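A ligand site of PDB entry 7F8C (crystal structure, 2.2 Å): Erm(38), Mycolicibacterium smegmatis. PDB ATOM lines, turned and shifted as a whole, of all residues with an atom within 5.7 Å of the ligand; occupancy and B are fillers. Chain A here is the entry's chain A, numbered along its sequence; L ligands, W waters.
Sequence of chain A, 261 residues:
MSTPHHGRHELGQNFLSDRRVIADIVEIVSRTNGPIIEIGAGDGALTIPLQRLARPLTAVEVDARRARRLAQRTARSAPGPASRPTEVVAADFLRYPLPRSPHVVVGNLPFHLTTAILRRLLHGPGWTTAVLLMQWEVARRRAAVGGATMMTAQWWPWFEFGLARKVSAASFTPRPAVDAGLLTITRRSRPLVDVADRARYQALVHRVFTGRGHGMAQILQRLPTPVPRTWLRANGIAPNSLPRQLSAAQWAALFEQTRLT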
ATOM      1  N   GLN A  13      14.796  -3.533  17.089  1.00  0.00           N
ATOM      2  CA  GLN A  13      14.312  -2.937  15.845  1.00  0.00           C
ATOM      3  C   GLN A  13      15.401  -3.000  14.776  1.00  0.00           C
ATOM      4  O   GLN A  13      16.591  -2.918  15.092  1.00  0.00           O
ATOM      5  CB  GLN A  13      13.832  -1.488  16.085  1.00  0.00           C
ATOM      6  CG  GLN A  13      12.784  -1.356  17.198  1.00  0.00           C
ATOM      7  CD  GLN A  13      11.390  -1.790  16.788  1.00  0.00           C
ATOM      8  OE1 GLN A  13      11.139  -2.174  15.641  1.00  0.00           O
ATOM      9  NE2 GLN A  13      10.442  -1.724  17.714  1.00  0.00           N
ATOM     10  N   ASN A  14      15.000  -3.175  13.503  1.00  0.00           N
ATOM     11  CA  ASN A  14      15.958  -3.300  12.408  1.00  0.00           C
ATOM     12  C   ASN A  14      15.829  -2.139  11.438  1.00  0.00           C
ATOM     13  O   ASN A  14      14.889  -2.068  10.644  1.00  0.00           O
ATOM     14  CB  ASN A  14      15.782  -4.635  11.681  1.00  0.00           C
ATOM     15  CG  ASN A  14      15.660  -5.816  12.589  1.00  0.00           C
ATOM     16  OD1 ASN A  14      14.575  -6.368  12.756  1.00  0.00           O
ATOM     17  ND2 ASN A  14      16.766  -6.212  13.209  1.00  0.00           N
ATOM     18  N   PHE A  15      16.813  -1.246  11.514  1.00  0.00           N
ATOM     19  CA  PHE A  15      16.871  -0.042  10.719  1.00  0.00           C
ATOM     20  C   PHE A  15      17.421  -0.362   9.331  1.00  0.00           C
ATOM     21  O   PHE A  15      18.235  -1.248   9.170  1.00  0.00           O
ATOM     22  CB  PHE A  15      17.704   1.034  11.469  1.00  0.00           C
ATOM     23  CG  PHE A  15      17.055   1.461  12.768  1.00  0.00           C
ATOM     24  CD1 PHE A  15      17.068   0.638  13.875  1.00  0.00           C
ATOM     25  CD2 PHE A  15      16.425   2.680  12.885  1.00  0.00           C
ATOM     26  CE1 PHE A  15      16.409   1.011  15.055  1.00  0.00           C
ATOM     27  CE2 PHE A  15      15.782   3.060  14.065  1.00  0.00           C
ATOM     28  CZ  PHE A  15      15.777   2.216  15.131  1.00  0.00           C
ATOM     29  N   LEU A  16      16.922   0.342   8.326  1.00  0.00           N
ATOM     30  CA  LEU A  16      17.343   0.120   6.961  1.00  0.00           C
ATOM     31  C   LEU A  16      18.696   0.789   6.715  1.00  0.00           C
ATOM     32  O   LEU A  16      18.770   2.028   6.700  1.00  0.00           O
ATOM     33  CB  LEU A  16      16.267   0.632   6.008  1.00  0.00           C
ATOM     34  CG  LEU A  16      16.387   0.301   4.510  1.00  0.00           C
ATOM     35  CD1 LEU A  16      16.611  -1.195   4.270  1.00  0.00           C
ATOM     36  CD2 LEU A  16      15.168   0.806   3.758  1.00  0.00           C
ATOM     37  N   GLU A  38       4.583   7.924   6.613  1.00  0.00           N
ATOM     38  CA  GLU A  38       5.577   6.901   6.860  1.00  0.00           C
ATOM     39  C   GLU A  38       5.405   6.276   8.226  1.00  0.00           C
ATOM     40  O   GLU A  38       5.210   6.992   9.186  1.00  0.00           O
ATOM     41  CB  GLU A  38       6.972   7.448   6.676  1.00  0.00           C
ATOM     42  CG  GLU A  38       8.057   6.388   6.871  1.00  0.00           C
ATOM     43  CD  GLU A  38       9.450   6.944   7.050  1.00  0.00           C
ATOM     44  OE1 GLU A  38       9.596   8.180   7.139  1.00  0.00           O
ATOM     45  OE2 GLU A  38      10.395   6.129   7.136  1.00  0.00           O
ATOM     46  N   ILE A  39       5.436   4.926   8.309  1.00  0.00           N
ATOM     47  CA  ILE A  39       5.313   4.163   9.569  1.00  0.00           C
ATOM     48  C   ILE A  39       6.706   3.749  10.020  1.00  0.00           C
ATOM     49  O   ILE A  39       7.460   3.174   9.225  1.00  0.00           O
ATOM     50  CB  ILE A  39       4.508   2.859   9.324  1.00  0.00           C
ATOM     51  CG1 ILE A  39       3.202   3.082   8.544  1.00  0.00           C
ATOM     52  CG2 ILE A  39       4.260   2.097  10.616  1.00  0.00           C
ATOM     53  CD1 ILE A  39       2.632   1.727   8.017  1.00  0.00           C
ATOM     54  N   GLY A  40       7.001   3.980  11.294  1.00  0.00           N
ATOM     55  CA  GLY A  40       8.290   3.594  11.871  1.00  0.00           C
ATOM     56  C   GLY A  40       9.435   4.349  11.245  1.00  0.00           C
ATOM     57  O   GLY A  40      10.348   3.740  10.706  1.00  0.00           O
ATOM     58  N   ALA A  41       9.373   5.659  11.264  1.00  0.00           N
ATOM     59  CA  ALA A  41      10.359   6.522  10.633  1.00  0.00           C
ATOM     60  C   ALA A  41      11.771   6.406  11.195  1.00  0.00           C
ATOM     61  O   ALA A  41      12.735   6.609  10.466  1.00  0.00           O
ATOM     62  CB  ALA A  41       9.880   7.955  10.664  1.00  0.00           C
ATOM     63  N   GLY A  42      11.900   5.981  12.454  1.00  0.00           N
ATOM     64  CA  GLY A  42      13.186   5.769  13.104  1.00  0.00           C
ATOM     65  C   GLY A  42      14.058   7.008  13.129  1.00  0.00           C
ATOM     66  O   GLY A  42      13.618   8.076  13.535  1.00  0.00           O
ATOM     67  N   ASP A  43      15.291   6.872  12.646  1.00  0.00           N
ATOM     68  CA  ASP A  43      16.214   7.985  12.521  1.00  0.00           C
ATOM     69  C   ASP A  43      16.068   8.772  11.237  1.00  0.00           C
ATOM     70  O   ASP A  43      16.781   9.757  11.079  1.00  0.00           O
ATOM     71  CB  ASP A  43      17.667   7.529  12.683  1.00  0.00           C
ATOM     72  CG  ASP A  43      18.004   7.066  14.081  1.00  0.00           C
ATOM     73  OD1 ASP A  43      17.360   7.552  15.038  1.00  0.00           O
ATOM     74  OD2 ASP A  43      18.915   6.234  14.224  1.00  0.00           O
ATOM     75  N   GLY A  44      15.172   8.351  10.338  1.00  0.00           N
ATOM     76  CA  GLY A  44      14.952   9.051   9.092  1.00  0.00           C
ATOM     77  C   GLY A  44      15.669   8.511   7.887  1.00  0.00           C
ATOM     78  O   GLY A  44      15.854   9.245   6.910  1.00  0.00           O
ATOM     79  N   ALA A  45      16.007   7.217   7.896  1.00  0.00           N
ATOM     80  CA  ALA A  45      16.678   6.540   6.767  1.00  0.00           C
ATOM     81  C   ALA A  45      15.845   6.673   5.488  1.00  0.00           C
ATOM     82  O   ALA A  45      16.410   6.895   4.425  1.00  0.00           O
ATOM     83  CB  ALA A  45      16.911   5.053   7.078  1.00  0.00           C
ATOM     84  N   LEU A  46      14.510   6.601   5.606  1.00  0.00           N
ATOM     85  CA  LEU A  46      13.618   6.835   4.466  1.00  0.00           C
ATOM     86  C   LEU A  46      13.041   8.249   4.504  1.00  0.00           C
ATOM     87  O   LEU A  46      12.852   8.856   3.455  1.00  0.00           O
ATOM     88  CB  LEU A  46      12.469   5.817   4.421  1.00  0.00           C
ATOM     89  CG  LEU A  46      12.869   4.375   4.099  1.00  0.00           C
ATOM     90  CD1 LEU A  46      11.667   3.435   4.286  1.00  0.00           C
ATOM     91  CD2 LEU A  46      13.442   4.281   2.707  1.00  0.00           C
ATOM     92  N   VAL A  60       5.789   8.909  11.247  1.00  0.00           N
ATOM     93  CA  VAL A  60       5.340   8.353  12.525  1.00  0.00           C
ATOM     94  C   VAL A  60       6.398   7.482  13.182  1.00  0.00           C
ATOM     95  O   VAL A  60       6.920   6.564  12.556  1.00  0.00           O
ATOM     96  CB  VAL A  60       3.991   7.607  12.353  1.00  0.00           C
ATOM     97  CG1 VAL A  60       3.481   7.078  13.686  1.00  0.00           C
ATOM     98  CG2 VAL A  60       2.954   8.517  11.721  1.00  0.00           C
ATOM     99  N   GLU A  61       6.756   7.786  14.431  1.00  0.00           N
ATOM    100  CA  GLU A  61       7.771   7.064  15.165  1.00  0.00           C
ATOM    101  C   GLU A  61       7.297   6.945  16.628  1.00  0.00           C
ATOM    102  O   GLU A  61       7.028   7.948  17.253  1.00  0.00           O
ATOM    103  CB  GLU A  61       9.115   7.809  15.056  1.00  0.00           C
ATOM    104  CG  GLU A  61      10.234   7.310  15.955  1.00  0.00           C
ATOM    105  CD  GLU A  61      10.477   5.824  15.898  1.00  0.00           C
ATOM    106  OE1 GLU A  61      10.505   5.257  14.783  1.00  0.00           O
ATOM    107  OE2 GLU A  61      10.598   5.202  16.973  1.00  0.00           O
ATOM    108  N   VAL A  62       7.161   5.717  17.140  1.00  0.00           N
ATOM    109  CA  VAL A  62       6.645   5.469  18.491  1.00  0.00           C
ATOM    110  C   VAL A  62       7.649   5.913  19.608  1.00  0.00           C
ATOM    111  O   VAL A  62       7.190   6.384  20.649  1.00  0.00           O
ATOM    112  CB  VAL A  62       6.143   4.005  18.626  1.00  0.00           C
ATOM    113  CG1 VAL A  62       7.292   3.008  18.697  1.00  0.00           C
ATOM    114  CG2 VAL A  62       5.206   3.836  19.816  1.00  0.00           C
ATOM    115  N   ASP A  63       8.976   5.809  19.385  1.00  0.00           N
ATOM    116  CA  ASP A  63       9.972   6.278  20.359  1.00  0.00           C
ATOM    117  C   ASP A  63      10.038   7.814  20.330  1.00  0.00           C
ATOM    118  O   ASP A  63      10.596   8.382  19.388  1.00  0.00           O
ATOM    119  CB  ASP A  63      11.354   5.670  20.047  1.00  0.00           C
ATOM    120  CG  ASP A  63      12.477   6.062  21.004  1.00  0.00           C
ATOM    121  OD1 ASP A  63      12.449   7.187  21.533  1.00  0.00           O
ATOM    122  OD2 ASP A  63      13.407   5.261  21.192  1.00  0.00           O
ATOM    123  N   ARG A  66      13.573   9.515  19.966  1.00  0.00           N
ATOM    124  CA  ARG A  66      14.017   9.327  18.588  1.00  0.00           C
ATOM    125  C   ARG A  66      13.204  10.211  17.626  1.00  0.00           C
ATOM    126  O   ARG A  66      13.770  10.790  16.704  1.00  0.00           O
ATOM    127  CB  ARG A  66      13.930   7.848  18.223  1.00  0.00           C
ATOM    128  CG  ARG A  66      14.737   7.479  16.990  1.00  0.00           C
ATOM    129  CD  ARG A  66      14.702   5.988  16.737  1.00  0.00           C
ATOM    130  NE  ARG A  66      15.356   5.232  17.797  1.00  0.00           N
ATOM    131  CZ  ARG A  66      14.866   4.114  18.330  1.00  0.00           C
ATOM    132  NH1 ARG A  66      13.713   3.615  17.903  1.00  0.00           N
ATOM    133  NH2 ARG A  66      15.526   3.487  19.310  1.00  0.00           N
ATOM    134  N   ALA A  91       3.970   8.718  17.845  1.00  0.00           N
ATOM    135  CA  ALA A  91       2.737   7.971  18.057  1.00  0.00           C
ATOM    136  C   ALA A  91       2.879   6.498  17.677  1.00  0.00           C
ATOM    137  O   ALA A  91       3.795   6.121  16.943  1.00  0.00           O
ATOM    138  CB  ALA A  91       1.592   8.609  17.244  1.00  0.00           C
ATOM    139  N   ASP A  92       1.977   5.652  18.196  1.00  0.00           N
ATOM    140  CA  ASP A  92       1.897   4.246  17.820  1.00  0.00           C
ATOM    141  C   ASP A  92       1.015   4.242  16.569  1.00  0.00           C
ATOM    142  O   ASP A  92      -0.106   4.755  16.626  1.00  0.00           O
ATOM    143  CB  ASP A  92       1.208   3.447  18.941  1.00  0.00           C
ATOM    144  CG  ASP A  92       1.156   1.955  18.750  1.00  0.00           C
ATOM    145  OD1 ASP A  92       1.525   1.471  17.651  1.00  0.00           O
ATOM    146  OD2 ASP A  92       0.769   1.251  19.697  1.00  0.00           O
ATOM    147  N   PHE A  93       1.507   3.720  15.424  1.00  0.00           N
ATOM    148  CA  PHE A  93       0.746   3.714  14.173  1.00  0.00           C
ATOM    149  C   PHE A  93      -0.580   2.914  14.289  1.00  0.00           C
ATOM    150  O   PHE A  93      -1.572   3.260  13.628  1.00  0.00           O
ATOM    151  CB  PHE A  93       1.603   3.217  13.005  1.00  0.00           C
ATOM    152  CG  PHE A  93       0.853   3.225  11.692  1.00  0.00           C
ATOM    153  CD1 PHE A  93       0.703   4.407  10.981  1.00  0.00           C
ATOM    154  CD2 PHE A  93       0.238   2.080  11.212  1.00  0.00           C
ATOM    155  CE1 PHE A  93      -0.042   4.428   9.807  1.00  0.00           C
ATOM    156  CE2 PHE A  93      -0.520   2.117  10.060  1.00  0.00           C
ATOM    157  CZ  PHE A  93      -0.641   3.289   9.351  1.00  0.00           C
ATOM    158  N   LEU A  94      -0.607   1.906  15.161  1.00  0.00           N
ATOM    159  CA  LEU A  94      -1.809   1.132  15.433  1.00  0.00           C
ATOM    160  C   LEU A  94      -2.949   2.011  16.008  1.00  0.00           C
ATOM    161  O   LEU A  94      -4.109   1.661  15.850  1.00  0.00           O
ATOM    162  CB  LEU A  94      -1.516  -0.080  16.331  1.00  0.00           C
ATOM    163  CG  LEU A  94      -0.684  -1.172  15.626  1.00  0.00           C
ATOM    164  CD1 LEU A  94      -0.207  -2.238  16.584  1.00  0.00           C
ATOM    165  CD2 LEU A  94      -1.445  -1.779  14.429  1.00  0.00           C
ATOM    166  N   ASN A 108       9.019   0.615   6.917  1.00  0.00           N
ATOM    167  CA  ASN A 108       9.894  -0.507   7.231  1.00  0.00           C
ATOM    168  C   ASN A 108       9.244  -1.033   8.504  1.00  0.00           C
ATOM    169  O   ASN A 108       9.407  -0.430   9.564  1.00  0.00           O
ATOM    170  CB  ASN A 108      11.301  -0.049   7.560  1.00  0.00           C
ATOM    171  CG  ASN A 108      12.246  -1.203   7.871  1.00  0.00           C
ATOM    172  OD1 ASN A 108      11.907  -2.388   7.728  1.00  0.00           O
ATOM    173  ND2 ASN A 108      13.455  -0.879   8.293  1.00  0.00           N
ATOM    174  N   LEU A 109       8.433  -2.067   8.395  1.00  0.00           N
ATOM    175  CA  LEU A 109       7.652  -2.559   9.513  1.00  0.00           C
ATOM    176  C   LEU A 109       8.397  -3.397  10.519  1.00  0.00           C
ATOM    177  O   LEU A 109       9.188  -4.271  10.155  1.00  0.00           O
ATOM    178  CB  LEU A 109       6.426  -3.348   8.993  1.00  0.00           C
ATOM    179  CG  LEU A 109       5.556  -2.661   7.926  1.00  0.00           C
ATOM    180  CD1 LEU A 109       4.301  -3.472   7.684  1.00  0.00           C
ATOM    181  CD2 LEU A 109       5.184  -1.225   8.313  1.00  0.00           C
ATOM    182  N   PRO A 110       8.097  -3.199  11.831  1.00  0.00           N
ATOM    183  CA  PRO A 110       8.686  -4.096  12.845  1.00  0.00           C
ATOM    184  C   PRO A 110       8.086  -5.473  12.572  1.00  0.00           C
ATOM    185  O   PRO A 110       6.875  -5.584  12.453  1.00  0.00           O
ATOM    186  CB  PRO A 110       8.178  -3.510  14.180  1.00  0.00           C
ATOM    187  CG  PRO A 110       7.546  -2.208  13.861  1.00  0.00           C
ATOM    188  CD  PRO A 110       7.146  -2.231  12.415  1.00  0.00           C
ATOM    189  N   LEU A 113       5.072  -6.886  14.449  1.00  0.00           N
ATOM    190  CA  LEU A 113       3.782  -6.224  14.326  1.00  0.00           C
ATOM    191  C   LEU A 113       3.221  -6.178  12.887  1.00  0.00           C
ATOM    192  O   LEU A 113       2.196  -5.553  12.649  1.00  0.00           O
ATOM    193  CB  LEU A 113       3.867  -4.800  14.903  1.00  0.00           C
ATOM    194  CG  LEU A 113       4.077  -4.698  16.402  1.00  0.00           C
ATOM    195  CD1 LEU A 113       4.375  -3.270  16.808  1.00  0.00           C
ATOM    196  CD2 LEU A 113       2.884  -5.216  17.164  1.00  0.00           C
ATOM    197  N   ILE A 117      -0.286  -4.480  11.714  1.00  0.00           N
ATOM    198  CA  ILE A 117      -0.178  -3.247  10.921  1.00  0.00           C
ATOM    199  C   ILE A 117      -0.874  -3.423   9.575  1.00  0.00           C
ATOM    200  O   ILE A 117      -1.589  -2.521   9.137  1.00  0.00           O
ATOM    201  CB  ILE A 117       1.315  -2.838  10.793  1.00  0.00           C
ATOM    202  CG1 ILE A 117       1.849  -2.294  12.147  1.00  0.00           C
ATOM    203  CG2 ILE A 117       1.561  -1.827   9.657  1.00  0.00           C
ATOM    204  CD1 ILE A 117       3.362  -2.321  12.217  1.00  0.00           C
HETATM  205  N1  LIG L   1      12.619   3.628   9.125  1.00  0.00           N
HETATM  206  C1  LIG L   1      13.516   3.457  10.275  1.00  0.00           C
HETATM  207  C2  LIG L   1      14.914   3.225   9.720  1.00  0.00           C
HETATM  208  O1  LIG L   1      15.000   2.344   8.838  1.00  0.00           O
HETATM  209  O2  LIG L   1      15.791   4.103  10.040  1.00  0.00           O
HETATM  210  C3  LIG L   1      13.009   2.438  11.333  1.00  0.00           C
HETATM  211  C4  LIG L   1      12.838   0.988  10.890  1.00  0.00           C
HETATM  212  C5  LIG L   1      12.289  -0.005  11.991  1.00  0.00           C
HETATM  213  N2  LIG L   1      12.294  -1.385  11.482  1.00  0.00           N
HETATM  214  C6  LIG L   1      10.879   0.269  12.563  1.00  0.00           C
HETATM  215  C7  LIG L   1      10.658   1.579  13.331  1.00  0.00           C
HETATM  216  O3  LIG L   1       9.298   1.484  13.825  1.00  0.00           O
HETATM  217  C8  LIG L   1      11.554   1.697  14.575  1.00  0.00           C
HETATM  218  O4  LIG L   1      12.158   3.001  14.541  1.00  0.00           O
HETATM  219  C9  LIG L   1      10.554   1.632  15.757  1.00  0.00           C
HETATM  220  O5  LIG L   1      10.934   2.495  16.882  1.00  0.00           O
HETATM  221  C10 LIG L   1       9.284   2.144  15.096  1.00  0.00           C
HETATM  222  N3  LIG L   1       8.025   1.717  15.761  1.00  0.00           N
HETATM  223  C11 LIG L   1       7.839   0.485  16.217  1.00  0.00           C
HETATM  224  N4  LIG L   1       6.533   0.321  16.434  1.00  0.00           N
HETATM  225  C12 LIG L   1       5.900   1.382  15.947  1.00  0.00           C
HETATM  226  C13 LIG L   1       4.597   1.713  15.925  1.00  0.00           C
HETATM  227  N5  LIG L   1       3.760   0.802  16.416  1.00  0.00           N
HETATM  228  N6  LIG L   1       4.148   2.869  15.410  1.00  0.00           N
HETATM  229  C14 LIG L   1       5.076   3.838  14.763  1.00  0.00           C
HETATM  230  N7  LIG L   1       6.488   3.390  14.889  1.00  0.00           N
HETATM  231  C15 LIG L   1       6.819   2.184  15.391  1.00  0.00           C
HETATM  232  O   HOH W   1       9.907   3.460   7.638  1.00  0.00           O
HETATM  233  O   HOH W   2      18.919   5.027  10.046  1.00  0.00           O
HETATM  234  O   HOH W   3      11.875  -3.984  10.043  1.00  0.00           O
HETATM  235  O   HOH W   4      12.801   6.344   7.906  1.00  0.00           O
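The backbone NH (N) of Ala 41 sits at hydrogen-bond distance from the backbone carbonyl oxygen (O) of Val 60, at 2.9 Å. OE2 of Glu 61 is in salt-bridge range of NH1 of Arg 66, 3.6 Å away. The guanidinium group (NH2) of Arg 66 is in salt-bridge range of the side-chain carboxylate (OD2) of Asp 63 (3.3 Å). The backbone NH (N) of Gly 40 is in hydrogen-bond range of the backbone carbonyl oxygen (O) of Val 60 (2.9 Å). OE1 of Glu 61 sits at hydrogen-bond distance from N of Gly 42 (2.8 Å). The side-chain carboxylate (OD1) of Asp 92 lies close to the backbone NH (N) of Leu 94 (3.3 Å). The side-chain carboxylate (OE2) of Glu 61 is in hydrogen-bond range of the backbone NH (N) of Asp 63, at 3.0 Å. N of Val 62 lies close to O of Ala 91 (3.4 Å).
A nitrogen (N7) of the ligand sits at hydrogen-bond distance from the backbone NH (N) of Val 62 (3.3 Å). The side-chain carboxylate (OE2) of Glu 38 is in salt-bridge range of a nitrogen (N1) of the ligand. The backbone carbonyl oxygen (O) of Asn 14 is in hydrogen-bond range of a nitrogen (N2) of the ligand. OE2 of Glu 61 lies within hydrogen-bond range of O5 of the ligand, 2.7 Å away. N1 of the ligand is in hydrogen-bond range of O of Gly 40, at 2.8 Å. ND2 of Asn 108 sits close to N2 of the ligand. The side-chain carboxylate of Asp 92 is in hydrogen-bond range of a nitrogen (N5) of the ligand, 2.6 Å away. The backbone NH (N) of Leu 16 is in hydrogen-bond range of an oxygen (O1) of the ligand (2.8 Å). The backbone NH (N) of Phe 93 is in hydrogen-bond range of a nitrogen (N6) of the ligand, at 2.8 Å. The guanidinium group of Arg 66 lies within hydrogen-bond range of an oxygen (O5) of the ligand. N1 of the ligand sits close to O of Ala 41, 3.3 Å away.
Residues that only touch the ligand: Gln 13 (3.7 Å), Phe 15 (3.2 Å), Gly 42 (3.3 Å), Asp 43 (3.8 Å), Ala 45 (3.3 Å), Val 60 (3.8 Å), Ala 91 (3.4 Å) and Pro 110 (3.6 Å). Hydrophobic or aromatic side chains that line the ligand: Phe 15, Leu 16, Ala 45, Val 60, Val 62, Phe 93 and Pro 110. Along chain A the residues within 4 Å of the ligand span positions 13 to 110. The nearest printed residue that does not touch the ligand is Leu 113 (4.1 Å).
Water W4 lies within hydrogen-bond range of the side-chain carboxylate of Glu 38 (2.5 Å), the backbone carbonyl oxygen of Ala 41 (2.6 Å), the backbone NH of Leu 46 (2.9 Å), a nitrogen (N1) of the ligand (3.0 Å) and the backbone NH of Ala 45 (3.3 Å). Water W3 lies within hydrogen-bond range of O of Leu 109 (2.7 Å), OD1 of Asn 108 (2.8 Å) and N2 of the ligand (3.0 Å).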
